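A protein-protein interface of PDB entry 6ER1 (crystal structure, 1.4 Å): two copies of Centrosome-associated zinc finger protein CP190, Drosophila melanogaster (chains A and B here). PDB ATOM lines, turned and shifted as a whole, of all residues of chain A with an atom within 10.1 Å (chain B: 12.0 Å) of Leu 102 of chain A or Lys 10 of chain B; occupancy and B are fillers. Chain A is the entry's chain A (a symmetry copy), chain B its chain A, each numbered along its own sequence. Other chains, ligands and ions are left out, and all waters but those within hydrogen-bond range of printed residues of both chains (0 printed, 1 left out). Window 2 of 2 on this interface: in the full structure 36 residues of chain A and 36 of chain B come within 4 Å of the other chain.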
ATOM      1  N   PRO A  88      17.340  27.246 -11.939  1.00  0.00           N
ATOM      2  CA  PRO A  88      16.083  27.990 -11.982  1.00  0.00           C
ATOM      3  C   PRO A  88      15.966  28.976 -10.771  1.00  0.00           C
ATOM      4  O   PRO A  88      15.397  30.065 -10.974  1.00  0.00           O
ATOM      5  CB  PRO A  88      14.975  26.930 -11.957  1.00  0.00           C
ATOM      6  CG  PRO A  88      15.648  25.680 -12.143  1.00  0.00           C
ATOM      7  CD  PRO A  88      17.114  25.783 -12.057  1.00  0.00           C
ATOM      8  N   THR A  97      11.126  35.875 -12.014  1.00  0.00           N
ATOM      9  CA  THR A  97      10.430  34.853 -12.748  1.00  0.00           C
ATOM     10  C   THR A  97      11.083  33.504 -12.444  1.00  0.00           C
ATOM     11  O   THR A  97      12.315  33.372 -12.484  1.00  0.00           O
ATOM     12  CB  THR A  97      10.495  35.137 -14.250  1.00  0.00           C
ATOM     13  OG1 THR A  97       9.813  36.343 -14.562  1.00  0.00           O
ATOM     14  CG2 THR A  97       9.868  34.019 -15.030  1.00  0.00           C
ATOM     15  N   LEU A  98      10.253  32.519 -12.115  1.00  0.00           N
ATOM     16  CA  LEU A  98      10.695  31.137 -11.976  1.00  0.00           C
ATOM     17  C   LEU A  98      10.169  30.357 -13.189  1.00  0.00           C
ATOM     18  O   LEU A  98       8.963  30.291 -13.400  1.00  0.00           O
ATOM     19  CB  LEU A  98      10.130  30.496 -10.713  1.00  0.00           C
ATOM     20  CG  LEU A  98      10.617  29.071 -10.443  1.00  0.00           C
ATOM     21  CD1 LEU A  98      12.061  29.019  -9.980  1.00  0.00           C
ATOM     22  CD2 LEU A  98       9.679  28.318  -9.491  1.00  0.00           C
ATOM     23  N   GLU A  99      11.091  29.831 -13.997  1.00  0.00           N
ATOM     24  CA  GLU A  99      10.787  28.962 -15.151  1.00  0.00           C
ATOM     25  C   GLU A  99      11.091  27.538 -14.731  1.00  0.00           C
ATOM     26  O   GLU A  99      12.196  27.275 -14.248  1.00  0.00           O
ATOM     27  CB  GLU A  99      11.671  29.341 -16.325  1.00  0.00           C
ATOM     28  CG  GLU A  99      11.338  30.694 -16.923  1.00  0.00           C
ATOM     29  CD  GLU A  99      12.037  30.981 -18.247  1.00  0.00           C
ATOM     30  OE1 GLU A  99      12.619  30.071 -18.861  1.00  0.00           O
ATOM     31  OE2 GLU A  99      11.992  32.136 -18.691  1.00  0.00           O
ATOM     32  N   PHE A 100      10.153  26.615 -14.925  1.00  0.00           N
ATOM     33  CA  PHE A 100      10.295  25.279 -14.393  1.00  0.00           C
ATOM     34  C   PHE A 100       9.358  24.348 -15.131  1.00  0.00           C
ATOM     35  O   PHE A 100       8.285  24.733 -15.543  1.00  0.00           O
ATOM     36  CB  PHE A 100      10.005  25.226 -12.889  1.00  0.00           C
ATOM     37  CG  PHE A 100       8.579  25.520 -12.501  1.00  0.00           C
ATOM     38  CD1 PHE A 100       8.057  26.792 -12.606  1.00  0.00           C
ATOM     39  CD2 PHE A 100       7.740  24.520 -12.084  1.00  0.00           C
ATOM     40  CE1 PHE A 100       6.740  27.059 -12.261  1.00  0.00           C
ATOM     41  CE2 PHE A 100       6.431  24.771 -11.747  1.00  0.00           C
ATOM     42  CZ  PHE A 100       5.926  26.046 -11.831  1.00  0.00           C
ATOM     43  N   GLU A 101       9.759  23.095 -15.243  1.00  0.00           N
ATOM     44  CA  GLU A 101       8.827  22.043 -15.676  1.00  0.00           C
ATOM     45  C   GLU A 101       8.000  21.603 -14.486  1.00  0.00           C
ATOM     46  O   GLU A 101       8.547  21.525 -13.370  1.00  0.00           O
ATOM     47  CB  GLU A 101       9.554  20.895 -16.367  1.00  0.00           C
ATOM     48  CG  GLU A 101      10.195  21.334 -17.678  1.00  0.00           C
ATOM     49  CD  GLU A 101      10.744  20.193 -18.513  1.00  0.00           C
ATOM     50  OE1 GLU A 101      11.687  20.444 -19.288  1.00  0.00           O
ATOM     51  OE2 GLU A 101      10.226  19.057 -18.418  1.00  0.00           O
ATOM     52  N   LEU A 102       6.713  21.291 -14.679  1.00  0.00           N
ATOM     53  CA  LEU A 102       5.864  20.851 -13.578  1.00  0.00           C
ATOM     54  C   LEU A 102       6.432  19.696 -12.818  1.00  0.00           C
ATOM     55  O   LEU A 102       6.220  19.577 -11.611  1.00  0.00           O
ATOM     56  CB  LEU A 102       4.432  20.505 -14.029  1.00  0.00           C
ATOM     57  CG  LEU A 102       3.552  21.650 -14.430  1.00  0.00           C
ATOM     58  CD1 LEU A 102       2.249  21.099 -14.991  1.00  0.00           C
ATOM     59  CD2 LEU A 102       3.334  22.550 -13.217  1.00  0.00           C
ATOM     60  N   LYS A 103       7.127  18.777 -13.517  1.00  0.00           N
ATOM     61  CA  LYS A 103       7.687  17.660 -12.833  1.00  0.00           C
ATOM     62  C   LYS A 103       8.694  18.019 -11.706  1.00  0.00           C
ATOM     63  O   LYS A 103       9.002  17.221 -10.859  1.00  0.00           O
ATOM     64  CB  LYS A 103       8.328  16.703 -13.854  1.00  0.00           C
ATOM     65  CG  LYS A 103       9.604  17.149 -14.487  1.00  0.00           C
ATOM     66  CD  LYS A 103      10.126  16.109 -15.502  1.00  0.00           C
ATOM     67  CE  LYS A 103      11.639  16.199 -15.667  1.00  0.00           C
ATOM     68  NZ  LYS A 103      12.187  15.574 -16.915  1.00  0.00           N
ATOM     69  N   MET A 104       9.218  19.246 -11.802  1.00  0.00           N
ATOM     70  CA  MET A 104      10.142  19.753 -10.775  1.00  0.00           C
ATOM     71  C   MET A 104       9.440  20.532  -9.667  1.00  0.00           C
ATOM     72  O   MET A 104      10.203  21.017  -8.753  1.00  0.00           O
ATOM     73  CB  MET A 104      11.188  20.670 -11.456  1.00  0.00           C
ATOM     74  CG  MET A 104      12.192  19.932 -12.310  1.00  0.00           C
ATOM     75  SD  MET A 104      13.330  18.918 -11.376  1.00  0.00           S
ATOM     76  CE  MET A 104      14.106  20.118 -10.318  1.00  0.00           C
ATOM     77  N   TYR A 105       8.157  20.723  -9.692  1.00  0.00           N
ATOM     78  CA  TYR A 105       7.464  21.601  -8.698  1.00  0.00           C
ATOM     79  C   TYR A 105       7.809  21.114  -7.353  1.00  0.00           C
ATOM     80  O   TYR A 105       8.246  21.988  -6.470  1.00  0.00           O
ATOM     81  CB  TYR A 105       5.953  21.600  -8.914  1.00  0.00           C
ATOM     82  CG  TYR A 105       5.221  22.359  -7.851  1.00  0.00           C
ATOM     83  CD1 TYR A 105       5.203  23.741  -7.917  1.00  0.00           C
ATOM     84  CD2 TYR A 105       4.577  21.736  -6.840  1.00  0.00           C
ATOM     85  CE1 TYR A 105       4.519  24.459  -6.959  1.00  0.00           C
ATOM     86  CE2 TYR A 105       3.875  22.460  -5.853  1.00  0.00           C
ATOM     87  CZ  TYR A 105       3.855  23.835  -5.938  1.00  0.00           C
ATOM     88  OH  TYR A 105       3.152  24.520  -4.965  1.00  0.00           O
ATOM     89  N   GLY A 106       7.569  19.907  -6.942  1.00  0.00           N
ATOM     90  CA  GLY A 106       7.795  19.484  -5.593  1.00  0.00           C
ATOM     91  C   GLY A 106       9.197  19.525  -5.182  1.00  0.00           C
ATOM     92  O   GLY A 106       9.491  19.946  -4.002  1.00  0.00           O
ATOM     93  N   LYS A 107      10.157  19.273  -6.006  1.00  0.00           N
ATOM     94  CA  LYS A 107      11.528  19.311  -5.675  1.00  0.00           C
ATOM     95  C   LYS A 107      11.886  20.808  -5.421  1.00  0.00           C
ATOM     96  O   LYS A 107      12.690  21.060  -4.477  1.00  0.00           O
ATOM     97  CB  LYS A 107      12.398  18.762  -6.820  1.00  0.00           C
ATOM     98  CG  LYS A 107      13.793  18.390  -6.361  1.00  0.00           C
ATOM     99  CD  LYS A 107      14.647  17.633  -7.361  1.00  0.00           C
ATOM    100  CE  LYS A 107      16.020  17.387  -6.754  1.00  0.00           C
ATOM    101  NZ  LYS A 107      16.899  16.544  -7.616  1.00  0.00           N
ATOM    102  N   LEU A 108      11.434  21.690  -6.254  1.00  0.00           N
ATOM    103  CA  LEU A 108      11.730  23.129  -6.067  1.00  0.00           C
ATOM    104  C   LEU A 108      11.101  23.561  -4.779  1.00  0.00           C
ATOM    105  O   LEU A 108      11.791  24.378  -4.034  1.00  0.00           O
ATOM    106  CB  LEU A 108      11.239  23.928  -7.240  1.00  0.00           C
ATOM    107  CG  LEU A 108      12.094  23.764  -8.500  1.00  0.00           C
ATOM    108  CD1 LEU A 108      11.308  24.280  -9.707  1.00  0.00           C
ATOM    109  CD2 LEU A 108      13.413  24.545  -8.378  1.00  0.00           C
ATOM    110  N   LEU A 109       9.909  23.166  -4.422  1.00  0.00           N
ATOM    111  CA  LEU A 109       9.262  23.547  -3.155  1.00  0.00           C
ATOM    112  C   LEU A 109      10.041  22.994  -2.037  1.00  0.00           C
ATOM    113  O   LEU A 109      10.333  23.769  -1.042  1.00  0.00           O
ATOM    114  CB  LEU A 109       7.824  23.137  -3.156  1.00  0.00           C
ATOM    115  CG  LEU A 109       6.974  23.491  -2.006  1.00  0.00           C
ATOM    116  CD1 LEU A 109       7.089  24.962  -1.634  1.00  0.00           C
ATOM    117  CD2 LEU A 109       5.541  23.108  -2.206  1.00  0.00           C
ATOM    118  N   ARG A 110      10.474  21.759  -1.994  1.00  0.00           N
ATOM    119  CA  ARG A 110      11.272  21.223  -0.922  1.00  0.00           C
ATOM    120  C   ARG A 110      12.601  21.968  -0.829  1.00  0.00           C
ATOM    121  O   ARG A 110      13.072  22.208   0.341  1.00  0.00           O
ATOM    122  CB  ARG A 110      11.470  19.695  -1.023  1.00  0.00           C
ATOM    123  CG  ARG A 110      10.169  18.938  -0.786  1.00  0.00           C
ATOM    124  CD  ARG A 110      10.350  17.416  -0.875  1.00  0.00           C
ATOM    125  NE  ARG A 110      10.723  16.910  -2.192  1.00  0.00           N
ATOM    126  CZ  ARG A 110       9.827  16.621  -3.128  1.00  0.00           C
ATOM    127  NH1 ARG A 110       8.541  16.765  -2.935  1.00  0.00           N
ATOM    128  NH2 ARG A 110      10.292  16.114  -4.279  1.00  0.00           N
ATOM    129  N   LEU A 123       5.697  32.429  -3.729  1.00  0.00           N
ATOM    130  CA  LEU A 123       5.382  32.308  -5.152  1.00  0.00           C
ATOM    131  C   LEU A 123       4.859  30.888  -5.514  1.00  0.00           C
ATOM    132  O   LEU A 123       3.847  30.757  -6.212  1.00  0.00           O
ATOM    133  CB  LEU A 123       6.608  32.675  -5.962  1.00  0.00           C
ATOM    134  CG  LEU A 123       6.439  32.550  -7.482  1.00  0.00           C
ATOM    135  CD1 LEU A 123       5.302  33.418  -8.001  1.00  0.00           C
ATOM    136  CD2 LEU A 123       7.733  32.858  -8.182  1.00  0.00           C
ATOM    137  N   LEU A 124       5.539  29.871  -5.007  1.00  0.00           N
ATOM    138  CA  LEU A 124       5.192  28.468  -5.380  1.00  0.00           C
ATOM    139  C   LEU A 124       3.877  28.086  -4.780  1.00  0.00           C
ATOM    140  O   LEU A 124       3.174  27.227  -5.321  1.00  0.00           O
ATOM    141  CB  LEU A 124       6.288  27.565  -4.894  1.00  0.00           C
ATOM    142  CG  LEU A 124       7.559  27.582  -5.744  1.00  0.00           C
ATOM    143  CD1 LEU A 124       8.635  26.831  -4.993  1.00  0.00           C
ATOM    144  CD2 LEU A 124       7.363  27.002  -7.127  1.00  0.00           C
ATOM    145  N   GLU B   8       6.035  20.562 -20.539  1.00  0.00           N
ATOM    146  CA  GLU B   8       6.539  21.845 -21.086  1.00  0.00           C
ATOM    147  C   GLU B   8       7.008  22.760 -19.950  1.00  0.00           C
ATOM    148  O   GLU B   8       6.708  22.538 -18.764  1.00  0.00           O
ATOM    149  CB  GLU B   8       5.459  22.601 -21.869  1.00  0.00           C
ATOM    150  CG  GLU B   8       4.452  23.381 -20.998  1.00  0.00           C
ATOM    151  CD  GLU B   8       3.416  24.138 -21.809  1.00  0.00           C
ATOM    152  OE1 GLU B   8       2.816  25.070 -21.235  1.00  0.00           O
ATOM    153  OE2 GLU B   8       3.204  23.815 -23.000  1.00  0.00           O
ATOM    154  N   VAL B   9       7.703  23.823 -20.335  1.00  0.00           N
ATOM    155  CA  VAL B   9       8.244  24.770 -19.371  1.00  0.00           C
ATOM    156  C   VAL B   9       7.167  25.781 -18.955  1.00  0.00           C
ATOM    157  O   VAL B   9       6.596  26.480 -19.800  1.00  0.00           O
ATOM    158  CB  VAL B   9       9.469  25.504 -19.952  1.00  0.00           C
ATOM    159  CG1 VAL B   9       9.985  26.557 -18.979  1.00  0.00           C
ATOM    160  CG2 VAL B   9      10.566  24.499 -20.296  1.00  0.00           C
ATOM    161  N   LYS B  10       6.905  25.861 -17.658  1.00  0.00           N
ATOM    162  CA  LYS B  10       5.991  26.854 -17.089  1.00  0.00           C
ATOM    163  C   LYS B  10       6.748  28.031 -16.501  1.00  0.00           C
ATOM    164  O   LYS B  10       7.946  27.967 -16.255  1.00  0.00           O
ATOM    165  CB  LYS B  10       5.150  26.222 -15.977  1.00  0.00           C
ATOM    166  CG  LYS B  10       4.467  24.916 -16.310  1.00  0.00           C
ATOM    167  CD  LYS B  10       3.574  25.005 -17.504  1.00  0.00           C
ATOM    168  CE  LYS B  10       2.668  23.800 -17.583  1.00  0.00           C
ATOM    169  NZ  LYS B  10       1.737  24.069 -18.686  1.00  0.00           N
ATOM    170  N   SER B  11       6.020  29.113 -16.277  1.00  0.00           N
ATOM    171  CA  SER B  11       6.623  30.221 -15.594  1.00  0.00           C
ATOM    172  C   SER B  11       5.621  30.950 -14.721  1.00  0.00           C
ATOM    173  O   SER B  11       4.454  31.084 -15.080  1.00  0.00           O
ATOM    174  CB  SER B  11       7.305  31.135 -16.607  1.00  0.00           C
ATOM    175  OG  SER B  11       6.506  32.204 -16.957  1.00  0.00           O
ATOM    176  N   VAL B  12       6.100  31.350 -13.543  1.00  0.00           N
ATOM    177  CA  VAL B  12       5.317  32.144 -12.592  1.00  0.00           C
ATOM    178  C   VAL B  12       6.247  33.271 -12.135  1.00  0.00           C
ATOM    179  O   VAL B  12       7.486  33.127 -12.215  1.00  0.00           O
ATOM    180  CB  VAL B  12       4.776  31.322 -11.410  1.00  0.00           C
ATOM    181  CG1 VAL B  12       3.770  30.276 -11.861  1.00  0.00           C
ATOM    182  CG2 VAL B  12       5.902  30.653 -10.628  1.00  0.00           C
ATOM    183  N   LYS B  13       5.677  34.392 -11.690  1.00  0.00           N
ATOM    184  CA  LYS B  13       6.489  35.550 -11.373  1.00  0.00           C
ATOM    185  C   LYS B  13       5.972  36.320 -10.169  1.00  0.00           C
ATOM    186  O   LYS B  13       4.767  36.321  -9.865  1.00  0.00           O
ATOM    187  CB  LYS B  13       6.627  36.496 -12.561  1.00  0.00           C
ATOM    188  CG  LYS B  13       5.364  37.158 -13.053  1.00  0.00           C
ATOM    189  CD  LYS B  13       5.635  37.988 -14.309  1.00  0.00           C
ATOM    190  CE  LYS B  13       4.753  39.230 -14.379  1.00  0.00           C
ATOM    191  NZ  LYS B  13       5.299  40.398 -13.607  1.00  0.00           N
ATOM    192  N   VAL B  14       6.912  36.989  -9.490  1.00  0.00           N
ATOM    193  CA  VAL B  14       6.611  37.979  -8.461  1.00  0.00           C
ATOM    194  C   VAL B  14       6.636  39.341  -9.166  1.00  0.00           C
ATOM    195  O   VAL B  14       7.633  39.721  -9.772  1.00  0.00           O
ATOM    196  CB  VAL B  14       7.677  37.953  -7.336  1.00  0.00           C
ATOM    197  CG1 VAL B  14       7.486  39.090  -6.328  1.00  0.00           C
ATOM    198  CG2 VAL B  14       7.656  36.619  -6.626  1.00  0.00           C
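Among the printed residues, pairs that only touch across the chains: Thr 97 of chain A with Val 12 of chain B (3.5 Å), Thr 97 of chain A with Lys 13 of chain B (3.8 Å), Leu 98 of chain A with Lys 10 of chain B (3.8 Å), Leu 98 of chain A with Ser 11 of chain B (3.2 Å), Glu 99 of chain A with Lys 10 of chain B (3.2 Å), Phe 100 of chain A with Val 9 of chain B (3.7 Å), Glu 101 of chain A with Glu 8 of chain B (3.8 Å), Leu 102 of chain A with Lys 10 of chain B (3.8 Å), Leu 123 of chain A with Val 12 of chain B (3.7 Å) and Leu 123 of chain A with Lys 13 of chain B (3.5 Å).
Of the 17 printed residues of chain A, 7 touch a printed residue of chain B.
Printed residues of chain A that touch a printed residue of chain B: Thr 97, Leu 98, Glu 99, Phe 100, Glu 101, Leu 102 and Leu 123.
Hydrophobic or aromatic side chains of chain A that line the printed part of chain B: Phe 100, Leu 102 and Leu 123.
Of the 7 printed residues of chain B, 6 touch a printed residue of chain A.
Printed residues of chain B that touch a printed residue of chain A: Glu 8, Val 9, Lys 10, Ser 11, Val 12 and Lys 13.
Among the printed residues, 12 pairs touch across the chains.
Among the printed residues, no Asp or Glu carboxylate lies within 4 Å of a Lys or Arg side-chain nitrogen of the other chain.
OE1 of Glu 8 of chain B lies within salt-bridge range of NZ of Lys 10 of chain B (2.9 Å).
No position is printed for both chains.
Of the 12 pairs that touch across the chains among the printed residues, none has its exchanged pair printed and touching as well.
Lys 10 of chain B touches just these residues of chain A: Leu 98 (3.8 Å), Glu 99 (3.2 Å), Phe 100 (2.8 Å) and Leu 102 (3.8 Å).
Leu 98 of chain A touches just these residues of chain B: Lys 10 (3.8 Å), Ser 11 (3.2 Å) and Val 12 (2.8 Å).
Glu 99 of chain A touches one residue of chain B.
Phe 100 of chain A touches just these residues of chain B: Val 9 (3.7 Å) and Lys 10 (2.8 Å).
Of the printed residues of chain A, Val 12 of chain B touches Thr 97, Leu 98 and Leu 123.
Of the printed residues of chain A, Lys 13 of chain B touches Thr 97 and Leu 123.
Of the printed residues of chain B, Leu 123 of chain A touches Val 12 (3.7 Å) and Lys 13 (3.5 Å).
Of the printed residues of chain B, Thr 97 of chain A touches Val 12 (3.5 Å) and Lys 13 (3.8 Å).
The nearest residue of chain B that does not touch Leu 102 of chain A is Glu 8 of chain B (4.3 Å).
The nearest printed residue of chain A that does not touch Lys 10 of chain B is Glu 101 of chain A (4.7 Å).
The nearest printed residue of chain A that does not touch Lys 13 of chain B is Leu 98 of chain A (4.9 Å).
The backbone NH (N) of Lys 10 of chain B is in hydrogen-bond range of the backbone carbonyl oxygen (O) of Phe 100 of chain A (2.8 Å).
O of Val 12 of chain B is in hydrogen-bond range of N of Leu 98 of chain A.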
